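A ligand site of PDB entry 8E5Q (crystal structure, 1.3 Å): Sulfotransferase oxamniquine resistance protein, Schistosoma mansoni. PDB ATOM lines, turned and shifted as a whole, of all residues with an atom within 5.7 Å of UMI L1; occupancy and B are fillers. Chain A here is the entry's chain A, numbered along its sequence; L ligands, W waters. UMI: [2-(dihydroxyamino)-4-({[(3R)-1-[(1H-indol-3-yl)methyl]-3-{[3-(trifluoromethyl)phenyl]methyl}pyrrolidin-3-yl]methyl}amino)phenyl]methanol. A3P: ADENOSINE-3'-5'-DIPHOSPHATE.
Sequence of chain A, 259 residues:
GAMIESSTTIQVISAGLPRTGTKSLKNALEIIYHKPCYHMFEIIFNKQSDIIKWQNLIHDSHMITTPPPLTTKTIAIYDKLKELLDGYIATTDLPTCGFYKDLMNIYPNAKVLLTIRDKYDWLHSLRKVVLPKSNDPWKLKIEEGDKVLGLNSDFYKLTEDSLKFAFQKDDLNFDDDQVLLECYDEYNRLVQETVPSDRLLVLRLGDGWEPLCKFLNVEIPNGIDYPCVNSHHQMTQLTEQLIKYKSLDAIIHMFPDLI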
ATOM      1  N   PRO A  18     -22.705 -21.923  18.951  1.00  0.00           N
ATOM      2  CA  PRO A  18     -21.564 -22.839  18.805  1.00  0.00           C
ATOM      3  C   PRO A  18     -20.667 -22.787  20.036  1.00  0.00           C
ATOM      4  O   PRO A  18     -20.537 -21.741  20.678  1.00  0.00           O
ATOM      5  CB  PRO A  18     -20.826 -22.301  17.575  1.00  0.00           C
ATOM      6  CG  PRO A  18     -21.316 -20.887  17.423  1.00  0.00           C
ATOM      7  CD  PRO A  18     -22.727 -20.911  17.889  1.00  0.00           C
ATOM      8  N   ARG A  19     -20.057 -23.938  20.352  1.00  0.00           N
ATOM      9  CA  ARG A  19     -19.135 -24.089  21.475  1.00  0.00           C
ATOM     10  C   ARG A  19     -19.842 -24.088  22.826  1.00  0.00           C
ATOM     11  O   ARG A  19     -19.239 -23.762  23.855  1.00  0.00           O
ATOM     12  CB  ARG A  19     -17.940 -23.123  21.426  1.00  0.00           C
ATOM     13  CG  ARG A  19     -17.216 -23.035  20.080  1.00  0.00           C
ATOM     14  CD  ARG A  19     -16.887 -24.409  19.499  1.00  0.00           C
ATOM     15  NE  ARG A  19     -15.914 -25.098  20.350  1.00  0.00           N
ATOM     16  CZ  ARG A  19     -15.517 -26.347  20.200  1.00  0.00           C
ATOM     17  NH1 ARG A  19     -16.008 -27.111  19.238  1.00  0.00           N
ATOM     18  NH2 ARG A  19     -14.565 -26.841  21.011  1.00  0.00           N
ATOM     19  N   THR A  22     -23.060 -28.249  21.524  1.00  0.00           N
ATOM     20  CA  THR A  22     -24.047 -28.597  20.508  1.00  0.00           C
ATOM     21  C   THR A  22     -23.751 -29.935  19.856  1.00  0.00           C
ATOM     22  O   THR A  22     -24.691 -30.634  19.457  1.00  0.00           O
ATOM     23  CB  THR A  22     -24.142 -27.509  19.428  1.00  0.00           C
ATOM     24  OG1 THR A  22     -22.878 -27.388  18.752  1.00  0.00           O
ATOM     25  CG2 THR A  22     -24.565 -26.162  20.016  1.00  0.00           C
ATOM     26  N   HIS A  39     -26.317 -30.090  12.080  1.00  0.00           N
ATOM     27  CA  HIS A  39     -25.267 -29.447  12.861  1.00  0.00           C
ATOM     28  C   HIS A  39     -24.330 -28.972  11.768  1.00  0.00           C
ATOM     29  O   HIS A  39     -24.429 -29.454  10.641  1.00  0.00           O
ATOM     30  CB  HIS A  39     -24.584 -30.448  13.771  1.00  0.00           C
ATOM     31  CG  HIS A  39     -23.492 -29.873  14.613  1.00  0.00           C
ATOM     32  ND1 HIS A  39     -22.205 -29.676  14.144  1.00  0.00           N
ATOM     33  CD2 HIS A  39     -23.478 -29.477  15.914  1.00  0.00           C
ATOM     34  CE1 HIS A  39     -21.456 -29.168  15.105  1.00  0.00           C
ATOM     35  NE2 HIS A  39     -22.201 -29.047  16.189  1.00  0.00           N
ATOM     36  N   MET A  40     -23.420 -28.053  12.040  1.00  0.00           N
ATOM     37  CA  MET A  40     -22.582 -27.597  10.910  1.00  0.00           C
ATOM     38  C   MET A  40     -21.670 -28.705  10.389  1.00  0.00           C
ATOM     39  O   MET A  40     -21.230 -28.644   9.240  1.00  0.00           O
ATOM     40  CB  MET A  40     -21.769 -26.357  11.256  1.00  0.00           C
ATOM     41  CG  MET A  40     -21.540 -25.453  10.047  1.00  0.00           C
ATOM     42  SD  MET A  40     -22.256 -23.813  10.244  1.00  0.00           S
ATOM     43  CE  MET A  40     -21.057 -22.793   9.393  1.00  0.00           C
ATOM     44  N   PHE A  41     -21.288 -29.649  11.243  1.00  0.00           N
ATOM     45  CA  PHE A  41     -20.494 -30.777  10.774  1.00  0.00           C
ATOM     46  C   PHE A  41     -21.197 -31.411   9.593  1.00  0.00           C
ATOM     47  O   PHE A  41     -20.562 -31.876   8.659  1.00  0.00           O
ATOM     48  CB  PHE A  41     -20.306 -31.810  11.871  1.00  0.00           C
ATOM     49  CG  PHE A  41     -19.203 -31.493  12.839  1.00  0.00           C
ATOM     50  CD1 PHE A  41     -18.949 -30.191  13.231  1.00  0.00           C
ATOM     51  CD2 PHE A  41     -18.418 -32.501  13.369  1.00  0.00           C
ATOM     52  CE1 PHE A  41     -17.944 -29.898  14.121  1.00  0.00           C
ATOM     53  CE2 PHE A  41     -17.405 -32.219  14.260  1.00  0.00           C
ATOM     54  CZ  PHE A  41     -17.157 -30.914  14.640  1.00  0.00           C
ATOM     55  N   ILE A  43     -22.748 -29.899   7.360  1.00  0.00           N
ATOM     56  CA  ILE A  43     -22.414 -29.100   6.187  1.00  0.00           C
ATOM     57  C   ILE A  43     -21.001 -29.369   5.692  1.00  0.00           C
ATOM     58  O   ILE A  43     -20.771 -29.523   4.491  1.00  0.00           O
ATOM     59  CB  ILE A  43     -22.557 -27.587   6.485  1.00  0.00           C
ATOM     60  CG1 ILE A  43     -23.976 -27.273   6.961  1.00  0.00           C
ATOM     61  CG2 ILE A  43     -22.189 -26.755   5.263  1.00  0.00           C
ATOM     62  CD1 ILE A  43     -24.263 -25.793   7.089  1.00  0.00           C
ATOM     63  N   ILE A  44     -20.036 -29.460   6.592  1.00  0.00           N
ATOM     64  CA  ILE A  44     -18.646 -29.609   6.144  1.00  0.00           C
ATOM     65  C   ILE A  44     -18.198 -31.034   5.823  1.00  0.00           C
ATOM     66  O   ILE A  44     -17.492 -31.245   4.833  1.00  0.00           O
ATOM     67  CB  ILE A  44     -17.672 -28.994   7.173  1.00  0.00           C
ATOM     68  CG1 ILE A  44     -17.356 -27.570   6.727  1.00  0.00           C
ATOM     69  CG2 ILE A  44     -16.405 -29.819   7.293  1.00  0.00           C
ATOM     70  CD1 ILE A  44     -18.228 -27.116   5.579  1.00  0.00           C
ATOM     71  N   PHE A  45     -18.616 -32.014   6.608  1.00  0.00           N
ATOM     72  CA  PHE A  45     -18.155 -33.384   6.382  1.00  0.00           C
ATOM     73  C   PHE A  45     -19.102 -34.182   5.513  1.00  0.00           C
ATOM     74  O   PHE A  45     -18.845 -35.359   5.247  1.00  0.00           O
ATOM     75  CB  PHE A  45     -17.946 -34.090   7.721  1.00  0.00           C
ATOM     76  CG  PHE A  45     -16.971 -33.405   8.630  1.00  0.00           C
ATOM     77  CD1 PHE A  45     -15.602 -33.562   8.440  1.00  0.00           C
ATOM     78  CD2 PHE A  45     -17.409 -32.608   9.666  1.00  0.00           C
ATOM     79  CE1 PHE A  45     -14.701 -32.935   9.274  1.00  0.00           C
ATOM     80  CE2 PHE A  45     -16.506 -31.971  10.502  1.00  0.00           C
ATOM     81  CZ  PHE A  45     -15.148 -32.136  10.308  1.00  0.00           C
ATOM     82  N   ASP A  93     -26.544 -25.897  16.443  1.00  0.00           N
ATOM     83  CA  ASP A  93     -25.401 -25.080  16.031  1.00  0.00           C
ATOM     84  C   ASP A  93     -25.718 -24.075  14.918  1.00  0.00           C
ATOM     85  O   ASP A  93     -26.848 -23.982  14.430  1.00  0.00           O
ATOM     86  CB  ASP A  93     -24.268 -26.013  15.604  1.00  0.00           C
ATOM     87  CG  ASP A  93     -22.960 -25.607  16.196  1.00  0.00           C
ATOM     88  OD1 ASP A  93     -22.567 -24.440  16.006  1.00  0.00           O
ATOM     89  OD2 ASP A  93     -22.292 -26.467  16.817  1.00  0.00           O
ATOM     90  N   LEU A  94     -24.677 -23.372  14.480  1.00  0.00           N
ATOM     91  CA  LEU A  94     -24.840 -22.461  13.359  1.00  0.00           C
ATOM     92  C   LEU A  94     -25.046 -23.333  12.144  1.00  0.00           C
ATOM     93  O   LEU A  94     -24.509 -24.434  12.089  1.00  0.00           O
ATOM     94  CB  LEU A  94     -23.585 -21.617  13.179  1.00  0.00           C
ATOM     95  CG  LEU A  94     -23.147 -20.627  14.252  1.00  0.00           C
ATOM     96  CD1 LEU A  94     -21.836 -19.980  13.838  1.00  0.00           C
ATOM     97  CD2 LEU A  94     -24.219 -19.584  14.498  1.00  0.00           C
ATOM     98  N   PRO A  95     -25.805 -22.861  11.154  1.00  0.00           N
ATOM     99  CA  PRO A  95     -26.449 -21.557  11.011  1.00  0.00           C
ATOM    100  C   PRO A  95     -27.913 -21.526  11.443  1.00  0.00           C
ATOM    101  O   PRO A  95     -28.589 -20.521  11.206  1.00  0.00           O
ATOM    102  CB  PRO A  95     -26.373 -21.321   9.510  1.00  0.00           C
ATOM    103  CG  PRO A  95     -26.478 -22.687   8.917  1.00  0.00           C
ATOM    104  CD  PRO A  95     -25.989 -23.675   9.942  1.00  0.00           C
ATOM    105  N   VAL A 129     -11.659 -22.330  17.890  1.00  0.00           N
ATOM    106  CA  VAL A 129     -12.251 -23.291  16.979  1.00  0.00           C
ATOM    107  C   VAL A 129     -13.007 -22.632  15.839  1.00  0.00           C
ATOM    108  O   VAL A 129     -12.858 -23.037  14.690  1.00  0.00           O
ATOM    109  CB  VAL A 129     -13.147 -24.312  17.723  1.00  0.00           C
ATOM    110  CG1 VAL A 129     -13.839 -25.255  16.736  1.00  0.00           C
ATOM    111  CG2 VAL A 129     -12.355 -25.086  18.778  1.00  0.00           C
ATOM    112  N   VAL A 130     -13.797 -21.609  16.128  1.00  0.00           N
ATOM    113  CA  VAL A 130     -14.798 -21.096  15.185  1.00  0.00           C
ATOM    114  C   VAL A 130     -14.378 -19.766  14.585  1.00  0.00           C
ATOM    115  O   VAL A 130     -14.477 -19.568  13.370  1.00  0.00           O
ATOM    116  CB  VAL A 130     -16.175 -20.975  15.868  1.00  0.00           C
ATOM    117  CG1 VAL A 130     -17.228 -20.408  14.892  1.00  0.00           C
ATOM    118  CG2 VAL A 130     -16.596 -22.305  16.404  1.00  0.00           C
ATOM    119  N   LEU A 131     -13.915 -18.834  15.416  1.00  0.00           N
ATOM    120  CA  LEU A 131     -13.776 -17.433  15.035  1.00  0.00           C
ATOM    121  C   LEU A 131     -12.551 -16.833  15.713  1.00  0.00           C
ATOM    122  O   LEU A 131     -12.671 -16.004  16.619  1.00  0.00           O
ATOM    123  CB  LEU A 131     -15.035 -16.649  15.424  1.00  0.00           C
ATOM    124  CG  LEU A 131     -15.282 -15.270  14.800  1.00  0.00           C
ATOM    125  CD1 LEU A 131     -15.785 -15.366  13.382  1.00  0.00           C
ATOM    126  CD2 LEU A 131     -16.225 -14.438  15.665  1.00  0.00           C
ATOM    127  N   PRO A 132     -11.358 -17.221  15.289  1.00  0.00           N
ATOM    128  CA  PRO A 132     -10.165 -16.611  15.872  1.00  0.00           C
ATOM    129  C   PRO A 132     -10.063 -15.142  15.485  1.00  0.00           C
ATOM    130  O   PRO A 132     -10.577 -14.701  14.449  1.00  0.00           O
ATOM    131  CB  PRO A 132      -9.009 -17.430  15.285  1.00  0.00           C
ATOM    132  CG  PRO A 132      -9.555 -17.971  14.008  1.00  0.00           C
ATOM    133  CD  PRO A 132     -11.021 -18.205  14.241  1.00  0.00           C
ATOM    134  N   LYS A 139      -4.976 -18.473  14.013  1.00  0.00           N
ATOM    135  CA  LYS A 139      -5.799 -18.317  12.818  1.00  0.00           C
ATOM    136  C   LYS A 139      -5.101 -18.889  11.587  1.00  0.00           C
ATOM    137  O   LYS A 139      -5.746 -19.479  10.717  1.00  0.00           O
ATOM    138  CB  LYS A 139      -6.133 -16.844  12.589  1.00  0.00           C
ATOM    139  CG  LYS A 139      -7.016 -16.604  11.371  1.00  0.00           C
ATOM    140  CD  LYS A 139      -7.269 -15.121  11.128  1.00  0.00           C
ATOM    141  CE  LYS A 139      -8.164 -14.912   9.925  1.00  0.00           C
ATOM    142  NZ  LYS A 139      -8.699 -13.525   9.797  1.00  0.00           N
ATOM    143  N   ILE A 142      -5.690 -22.618  11.582  1.00  0.00           N
ATOM    144  CA  ILE A 142      -7.086 -22.924  11.290  1.00  0.00           C
ATOM    145  C   ILE A 142      -7.336 -22.792   9.803  1.00  0.00           C
ATOM    146  O   ILE A 142      -7.965 -23.662   9.197  1.00  0.00           O
ATOM    147  CB  ILE A 142      -8.038 -22.005  12.076  1.00  0.00           C
ATOM    148  CG1 ILE A 142      -8.029 -22.365  13.562  1.00  0.00           C
ATOM    149  CG2 ILE A 142      -9.451 -22.101  11.512  1.00  0.00           C
ATOM    150  CD1 ILE A 142      -9.038 -21.608  14.386  1.00  0.00           C
ATOM    151  N   GLU A 143      -6.831 -21.722   9.206  1.00  0.00           N
ATOM    152  CA  GLU A 143      -7.052 -21.512   7.779  1.00  0.00           C
ATOM    153  C   GLU A 143      -6.371 -22.583   6.936  1.00  0.00           C
ATOM    154  O   GLU A 143      -6.917 -23.000   5.906  1.00  0.00           O
ATOM    155  CB  GLU A 143      -6.596 -20.112   7.348  1.00  0.00           C
ATOM    156  CG  GLU A 143      -7.340 -18.984   8.025  1.00  0.00           C
ATOM    157  CD  GLU A 143      -6.817 -17.625   7.591  1.00  0.00           C
ATOM    158  OE1 GLU A 143      -5.572 -17.478   7.485  1.00  0.00           O
ATOM    159  OE2 GLU A 143      -7.631 -16.720   7.349  1.00  0.00           O
ATOM    160  N   ASP A 146      -8.457 -25.606   7.209  1.00  0.00           N
ATOM    161  CA  ASP A 146      -9.692 -25.394   6.462  1.00  0.00           C
ATOM    162  C   ASP A 146      -9.496 -25.724   4.986  1.00  0.00           C
ATOM    163  O   ASP A 146     -10.376 -26.336   4.362  1.00  0.00           O
ATOM    164  CB  ASP A 146     -10.124 -23.936   6.622  1.00  0.00           C
ATOM    165  CG  ASP A 146     -10.915 -23.694   7.894  1.00  0.00           C
ATOM    166  OD1 ASP A 146     -11.196 -24.667   8.621  1.00  0.00           O
ATOM    167  OD2 ASP A 146     -11.235 -22.530   8.179  1.00  0.00           O
ATOM    168  N   LEU A 149      -9.705 -29.312   4.362  1.00  0.00           N
ATOM    169  CA  LEU A 149     -11.083 -29.768   4.348  1.00  0.00           C
ATOM    170  C   LEU A 149     -11.872 -29.276   3.136  1.00  0.00           C
ATOM    171  O   LEU A 149     -13.027 -29.690   2.958  1.00  0.00           O
ATOM    172  CB  LEU A 149     -11.825 -29.381   5.630  1.00  0.00           C
ATOM    173  CG  LEU A 149     -11.238 -29.801   6.981  1.00  0.00           C
ATOM    174  CD1 LEU A 149     -11.852 -28.972   8.119  1.00  0.00           C
ATOM    175  CD2 LEU A 149     -11.396 -31.291   7.230  1.00  0.00           C
ATOM    176  N   LEU A 151     -12.689 -25.982   2.501  1.00  0.00           N
ATOM    177  CA  LEU A 151     -13.515 -24.844   2.875  1.00  0.00           C
ATOM    178  C   LEU A 151     -12.949 -23.552   2.301  1.00  0.00           C
ATOM    179  O   LEU A 151     -11.741 -23.309   2.404  1.00  0.00           O
ATOM    180  CB  LEU A 151     -13.591 -24.735   4.402  1.00  0.00           C
ATOM    181  CG  LEU A 151     -14.116 -26.011   5.024  1.00  0.00           C
ATOM    182  CD1 LEU A 151     -14.325 -25.848   6.532  1.00  0.00           C
ATOM    183  CD2 LEU A 151     -15.391 -26.342   4.313  1.00  0.00           C
ATOM    184  N   PHE A 155     -17.615 -20.218   3.143  1.00  0.00           N
ATOM    185  CA  PHE A 155     -17.835 -20.802   4.463  1.00  0.00           C
ATOM    186  C   PHE A 155     -17.524 -19.830   5.586  1.00  0.00           C
ATOM    187  O   PHE A 155     -18.201 -19.824   6.617  1.00  0.00           O
ATOM    188  CB  PHE A 155     -17.042 -22.081   4.627  1.00  0.00           C
ATOM    189  CG  PHE A 155     -17.539 -22.927   5.740  1.00  0.00           C
ATOM    190  CD1 PHE A 155     -18.753 -23.563   5.668  1.00  0.00           C
ATOM    191  CD2 PHE A 155     -16.833 -22.991   6.924  1.00  0.00           C
ATOM    192  CE1 PHE A 155     -19.214 -24.300   6.708  1.00  0.00           C
ATOM    193  CE2 PHE A 155     -17.289 -23.740   7.976  1.00  0.00           C
ATOM    194  CZ  PHE A 155     -18.475 -24.396   7.869  1.00  0.00           C
ATOM    195  N   TYR A 156     -16.460 -19.042   5.430  1.00  0.00           N
ATOM    196  CA  TYR A 156     -16.131 -18.069   6.464  1.00  0.00           C
ATOM    197  C   TYR A 156     -17.218 -17.011   6.568  1.00  0.00           C
ATOM    198  O   TYR A 156     -17.615 -16.631   7.672  1.00  0.00           O
ATOM    199  CB  TYR A 156     -14.799 -17.398   6.134  1.00  0.00           C
ATOM    200  CG  TYR A 156     -13.590 -18.291   6.290  1.00  0.00           C
ATOM    201  CD1 TYR A 156     -13.729 -19.663   6.356  1.00  0.00           C
ATOM    202  CD2 TYR A 156     -12.321 -17.756   6.360  1.00  0.00           C
ATOM    203  CE1 TYR A 156     -12.627 -20.485   6.494  1.00  0.00           C
ATOM    204  CE2 TYR A 156     -11.212 -18.571   6.512  1.00  0.00           C
ATOM    205  CZ  TYR A 156     -11.380 -19.928   6.580  1.00  0.00           C
ATOM    206  OH  TYR A 156     -10.291 -20.749   6.724  1.00  0.00           O
ATOM    207  N   LYS A 157     -17.715 -16.556   5.422  1.00  0.00           N
ATOM    208  CA  LYS A 157     -18.775 -15.559   5.434  1.00  0.00           C
ATOM    209  C   LYS A 157     -20.054 -16.155   6.013  1.00  0.00           C
ATOM    210  O   LYS A 157     -20.793 -15.463   6.722  1.00  0.00           O
ATOM    211  CB  LYS A 157     -18.983 -15.006   4.025  1.00  0.00           C
ATOM    212  CG  LYS A 157     -20.295 -14.291   3.804  1.00  0.00           C
ATOM    213  CD  LYS A 157     -20.185 -13.200   2.753  1.00  0.00           C
ATOM    214  CE  LYS A 157     -20.911 -13.588   1.472  1.00  0.00           C
ATOM    215  NZ  LYS A 157     -21.172 -12.423   0.587  1.00  0.00           N
ATOM    216  N   THR A 159     -20.192 -18.404   8.381  1.00  0.00           N
ATOM    217  CA  THR A 159     -20.002 -18.427   9.827  1.00  0.00           C
ATOM    218  C   THR A 159     -20.256 -17.045  10.414  1.00  0.00           C
ATOM    219  O   THR A 159     -21.004 -16.897  11.393  1.00  0.00           O
ATOM    220  CB  THR A 159     -18.570 -18.888  10.138  1.00  0.00           C
ATOM    221  OG1 THR A 159     -18.362 -20.200   9.607  1.00  0.00           O
ATOM    222  CG2 THR A 159     -18.364 -18.954  11.638  1.00  0.00           C
ATOM    223  N   GLU A 160     -19.648 -16.034   9.825  1.00  0.00           N
ATOM    224  CA  GLU A 160     -19.798 -14.677  10.339  1.00  0.00           C
ATOM    225  C   GLU A 160     -21.229 -14.202  10.200  1.00  0.00           C
ATOM    226  O   GLU A 160     -21.795 -13.647  11.145  1.00  0.00           O
ATOM    227  CB  GLU A 160     -18.854 -13.736   9.593  1.00  0.00           C
ATOM    228  CG  GLU A 160     -17.389 -13.852  10.026  1.00  0.00           C
ATOM    229  CD  GLU A 160     -16.456 -12.979   9.206  1.00  0.00           C
ATOM    230  OE1 GLU A 160     -16.943 -12.256   8.303  1.00  0.00           O
ATOM    231  OE2 GLU A 160     -15.224 -13.018   9.448  1.00  0.00           O
ATOM    232  N   ASN A 230     -16.070 -33.033  20.976  1.00  0.00           N
ATOM    233  CA  ASN A 230     -15.833 -31.766  20.307  1.00  0.00           C
ATOM    234  C   ASN A 230     -15.081 -30.763  21.182  1.00  0.00           C
ATOM    235  O   ASN A 230     -15.270 -29.556  21.060  1.00  0.00           O
ATOM    236  CB  ASN A 230     -17.136 -31.183  19.745  1.00  0.00           C
ATOM    237  CG  ASN A 230     -16.936 -30.399  18.481  1.00  0.00           C
ATOM    238  OD1 ASN A 230     -15.994 -30.655  17.728  1.00  0.00           O
ATOM    239  ND2 ASN A 230     -17.840 -29.473  18.199  1.00  0.00           N
ATOM    240  N   MET A 235     -10.193 -30.452  18.783  1.00  0.00           N
ATOM    241  CA  MET A 235     -10.142 -29.661  17.553  1.00  0.00           C
ATOM    242  C   MET A 235      -8.751 -29.127  17.250  1.00  0.00           C
ATOM    243  O   MET A 235      -8.356 -29.046  16.088  1.00  0.00           O
ATOM    244  CB  MET A 235     -11.210 -28.555  17.531  1.00  0.00           C
ATOM    245  CG  MET A 235     -12.654 -29.053  17.659  1.00  0.00           C
ATOM    246  SD  MET A 235     -13.060 -30.014  16.175  1.00  0.00           S
ATOM    247  CE  MET A 235     -12.726 -28.792  14.917  1.00  0.00           C
HETATM  248  C1  UMI L   1     -19.794 -24.175  12.199  1.00  0.00           C
HETATM  249  C10 UMI L   1     -14.291 -26.572  12.754  1.00  0.00           C
HETATM  250  C11 UMI L   1     -14.304 -22.588  10.523  1.00  0.00           C
HETATM  251  C12 UMI L   1     -16.393 -27.124  12.265  1.00  0.00           C
HETATM  252  C14 UMI L   1     -13.037 -22.582  11.346  1.00  0.00           C
HETATM  253  C15 UMI L   1     -12.597 -24.024  11.467  1.00  0.00           C
HETATM  254  C16 UMI L   1     -15.720 -26.856  10.995  1.00  0.00           C
HETATM  255  C17 UMI L   1     -14.474 -24.024  10.050  1.00  0.00           C
HETATM  256  C18 UMI L   1     -17.714 -27.460  12.219  1.00  0.00           C
HETATM  257  C19 UMI L   1     -18.321 -27.600  10.994  1.00  0.00           C
HETATM  258  C2  UMI L   1     -19.266 -24.664  13.394  1.00  0.00           C
HETATM  259  C20 UMI L   1     -17.682 -27.328   9.798  1.00  0.00           C
HETATM  260  C21 UMI L   1     -16.352 -26.952   9.777  1.00  0.00           C
HETATM  261  C22 UMI L   1     -14.249 -21.694   9.284  1.00  0.00           C
HETATM  262  C23 UMI L   1     -13.970 -20.240   9.595  1.00  0.00           C
HETATM  263  C24 UMI L   1     -15.019 -19.324   9.655  1.00  0.00           C
HETATM  264  C25 UMI L   1     -14.764 -17.985   9.935  1.00  0.00           C
HETATM  265  C26 UMI L   1     -13.457 -17.560  10.145  1.00  0.00           C
HETATM  266  C27 UMI L   1     -12.416 -18.473  10.082  1.00  0.00           C
HETATM  267  C28 UMI L   1     -12.667 -19.802   9.794  1.00  0.00           C
HETATM  268  C29 UMI L   1     -10.999 -18.026  10.300  1.00  0.00           C
HETATM  269  C3  UMI L   1     -17.958 -24.490  13.770  1.00  0.00           C
HETATM  270  C30 UMI L   1     -15.462 -22.191  11.438  1.00  0.00           C
HETATM  271  C4  UMI L   1     -17.092 -23.836  12.915  1.00  0.00           C
HETATM  272  C5  UMI L   1     -17.571 -23.325  11.717  1.00  0.00           C
HETATM  273  C6  UMI L   1     -18.906 -23.487  11.365  1.00  0.00           C
HETATM  274  C7  UMI L   1     -20.157 -25.362  14.364  1.00  0.00           C
HETATM  275  C8  UMI L   1     -13.229 -26.127  10.435  1.00  0.00           C
HETATM  276  C9  UMI L   1     -14.341 -26.499  11.372  1.00  0.00           C
HETATM  277  F30 UMI L   1     -10.523 -17.554   9.174  1.00  0.00           F
HETATM  278  F31 UMI L   1     -11.001 -17.074  11.217  1.00  0.00           F
HETATM  279  F32 UMI L   1     -10.272 -19.045  10.703  1.00  0.00           F
HETATM  280  N11 UMI L   1     -15.506 -26.939  13.251  1.00  0.00           N
HETATM  281  N12 UMI L   1     -16.718 -22.675  10.900  1.00  0.00           N
HETATM  282  N16 UMI L   1     -13.170 -24.666  10.276  1.00  0.00           N
HETATM  283  N8  UMI L   1     -17.505 -25.042  14.987  1.00  0.00           N
HETATM  284  O10 UMI L   1     -18.097 -24.775  16.224  1.00  0.00           O
HETATM  285  O11 UMI L   1     -16.418 -25.910  14.977  1.00  0.00           O
HETATM  286  O9  UMI L   1     -21.438 -25.006  13.850  1.00  0.00           O
HETATM  287  P1  A3P L   2     -14.175 -26.669  25.099  1.00  0.00           P
HETATM  288  O1P A3P L   2     -13.770 -26.022  23.711  1.00  0.00           O
HETATM  289  O2P A3P L   2     -13.992 -25.642  26.257  1.00  0.00           O
HETATM  290  O3P A3P L   2     -13.470 -27.960  25.295  1.00  0.00           O
HETATM  291  P2  A3P L   2     -19.814 -27.514  20.492  1.00  0.00           P
HETATM  292  O4P A3P L   2     -18.813 -26.881  19.438  1.00  0.00           O
HETATM  293  O5P A3P L   2     -21.170 -26.692  20.543  1.00  0.00           O
HETATM  294  O6P A3P L   2     -20.043 -28.949  20.201  1.00  0.00           O
HETATM  295  O5' A3P L   2     -19.294 -27.377  22.016  1.00  0.00           O
HETATM  296  C5' A3P L   2     -18.042 -28.007  22.343  1.00  0.00           C
HETATM  297  C4' A3P L   2     -17.657 -27.540  23.737  1.00  0.00           C
HETATM  298  O4' A3P L   2     -18.519 -28.175  24.723  1.00  0.00           O
HETATM  299  C3' A3P L   2     -16.233 -27.916  24.160  1.00  0.00           C
HETATM  300  O3' A3P L   2     -15.799 -26.903  25.096  1.00  0.00           O
HETATM  301  C2' A3P L   2     -16.460 -29.259  24.847  1.00  0.00           C
HETATM  302  O2' A3P L   2     -15.397 -29.656  25.706  1.00  0.00           O
HETATM  303  C1' A3P L   2     -17.725 -28.925  25.623  1.00  0.00           C
HETATM  304  N9  A3P L   2     -18.484 -30.091  26.048  1.00  0.00           N
HETATM  305  C8  A3P L   2     -19.237 -30.899  25.235  1.00  0.00           C
HETATM  306  N7  A3P L   2     -19.818 -31.888  25.856  1.00  0.00           N
HETATM  307  C5  A3P L   2     -19.428 -31.728  27.168  1.00  0.00           C
HETATM  308  C6  A3P L   2     -19.727 -32.460  28.339  1.00  0.00           C
HETATM  309  N6  A3P L   2     -20.506 -33.547  28.350  1.00  0.00           N
HETATM  310  N1  A3P L   2     -19.169 -32.036  29.502  1.00  0.00           N
HETATM  311  C2  A3P L   2     -18.377 -30.950  29.484  1.00  0.00           C
HETATM  312  N3  A3P L   2     -18.039 -30.183  28.447  1.00  0.00           N
HETATM  313  C4  A3P L   2     -18.598 -30.631  27.303  1.00  0.00           C
HETATM  314  O   HOH W   1     -11.298 -25.401  14.136  1.00  0.00           O
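An oxygen (O9) of UMI L1 is in hydrogen-bond range of the side-chain carboxylate (OD1) of Asp 93, 2.5 Å away. The side-chain carboxylate (OD1) of Asp 146 lies within salt-bridge range of a nitrogen (N16) of UMI L1. N12 of UMI L1 is in hydrogen-bond range of OG1 of Thr 159 (3.2 Å). N of Arg 19 is in hydrogen-bond range of O5P of A3P L2, 3.0 Å away. The guanidinium group (NH1) of Arg 19 lies within salt-bridge range of an oxygen (O4P) of A3P L2 (2.8 Å). The side-chain amide nitrogen (ND2) of Asn 230 lies within hydrogen-bond range of an oxygen (O6P) of A3P L2. An oxygen (O5P) of A3P L2 is in hydrogen-bond range of the backbone NH of Thr 22 (2.6 Å). The side-chain hydroxyl (OG1) of Thr 22 sits at hydrogen-bond distance from an oxygen (O5P) of A3P L2, at 2.6 Å.
OD2 of Asp 93 sits at hydrogen-bond distance from NE2 of His 39 (2.7 Å). The side-chain carboxylate (OD2) of Asp 146 is in hydrogen-bond range of the side-chain hydroxyl (OH) of Tyr 156, at 2.5 Å. The backbone carbonyl oxygen (O) of Asp 146 is in hydrogen-bond range of the backbone NH (N) of Leu 151 (3.0 Å). A ring nitrogen (ND1) of His 39 lies within hydrogen-bond range of the backbone NH of Phe 41 (3.0 Å). O of Phe 155 sits at hydrogen-bond distance from OG1 of Thr 159, 3.0 Å away. The side-chain sulfur (SD) of Met 235 sits close to the side-chain amide oxygen (OD1) of Asn 230 (3.4 Å). O of Asn 230 sits at hydrogen-bond distance from NH2 of Arg 19 (2.8 Å).
Residues that only touch UMI L1: Pro 18 (3.9 Å), Arg 19 (3.5 Å), Met 40 (2.9 Å), Phe 41 (3.1 Å), Ile 44 (3.1 Å), Leu 94 (3.6 Å), Val 129 (3.2 Å), Val 130 (2.9 Å), Pro 132 (3.2 Å), Lys 139 (3.6 Å), Ile 142 (3.3 Å), Glu 143 (3.5 Å), Leu 149 (3.9 Å), Leu 151 (3.97 Å), Phe 155 (3.2 Å), Tyr 156 (2.9 Å) and Met 235 (3.5 Å). Hydrophobic or aromatic side chains that line UMI L1: Pro 18, Met 40, Phe 41, Ile 44, Val 129, Val 130, Pro 132, Ile 142, Leu 149, Leu 151, Phe 155, Tyr 156 and Met 235. The nearest printed residue that does not touch UMI L1 is His 39 (4.1 Å).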
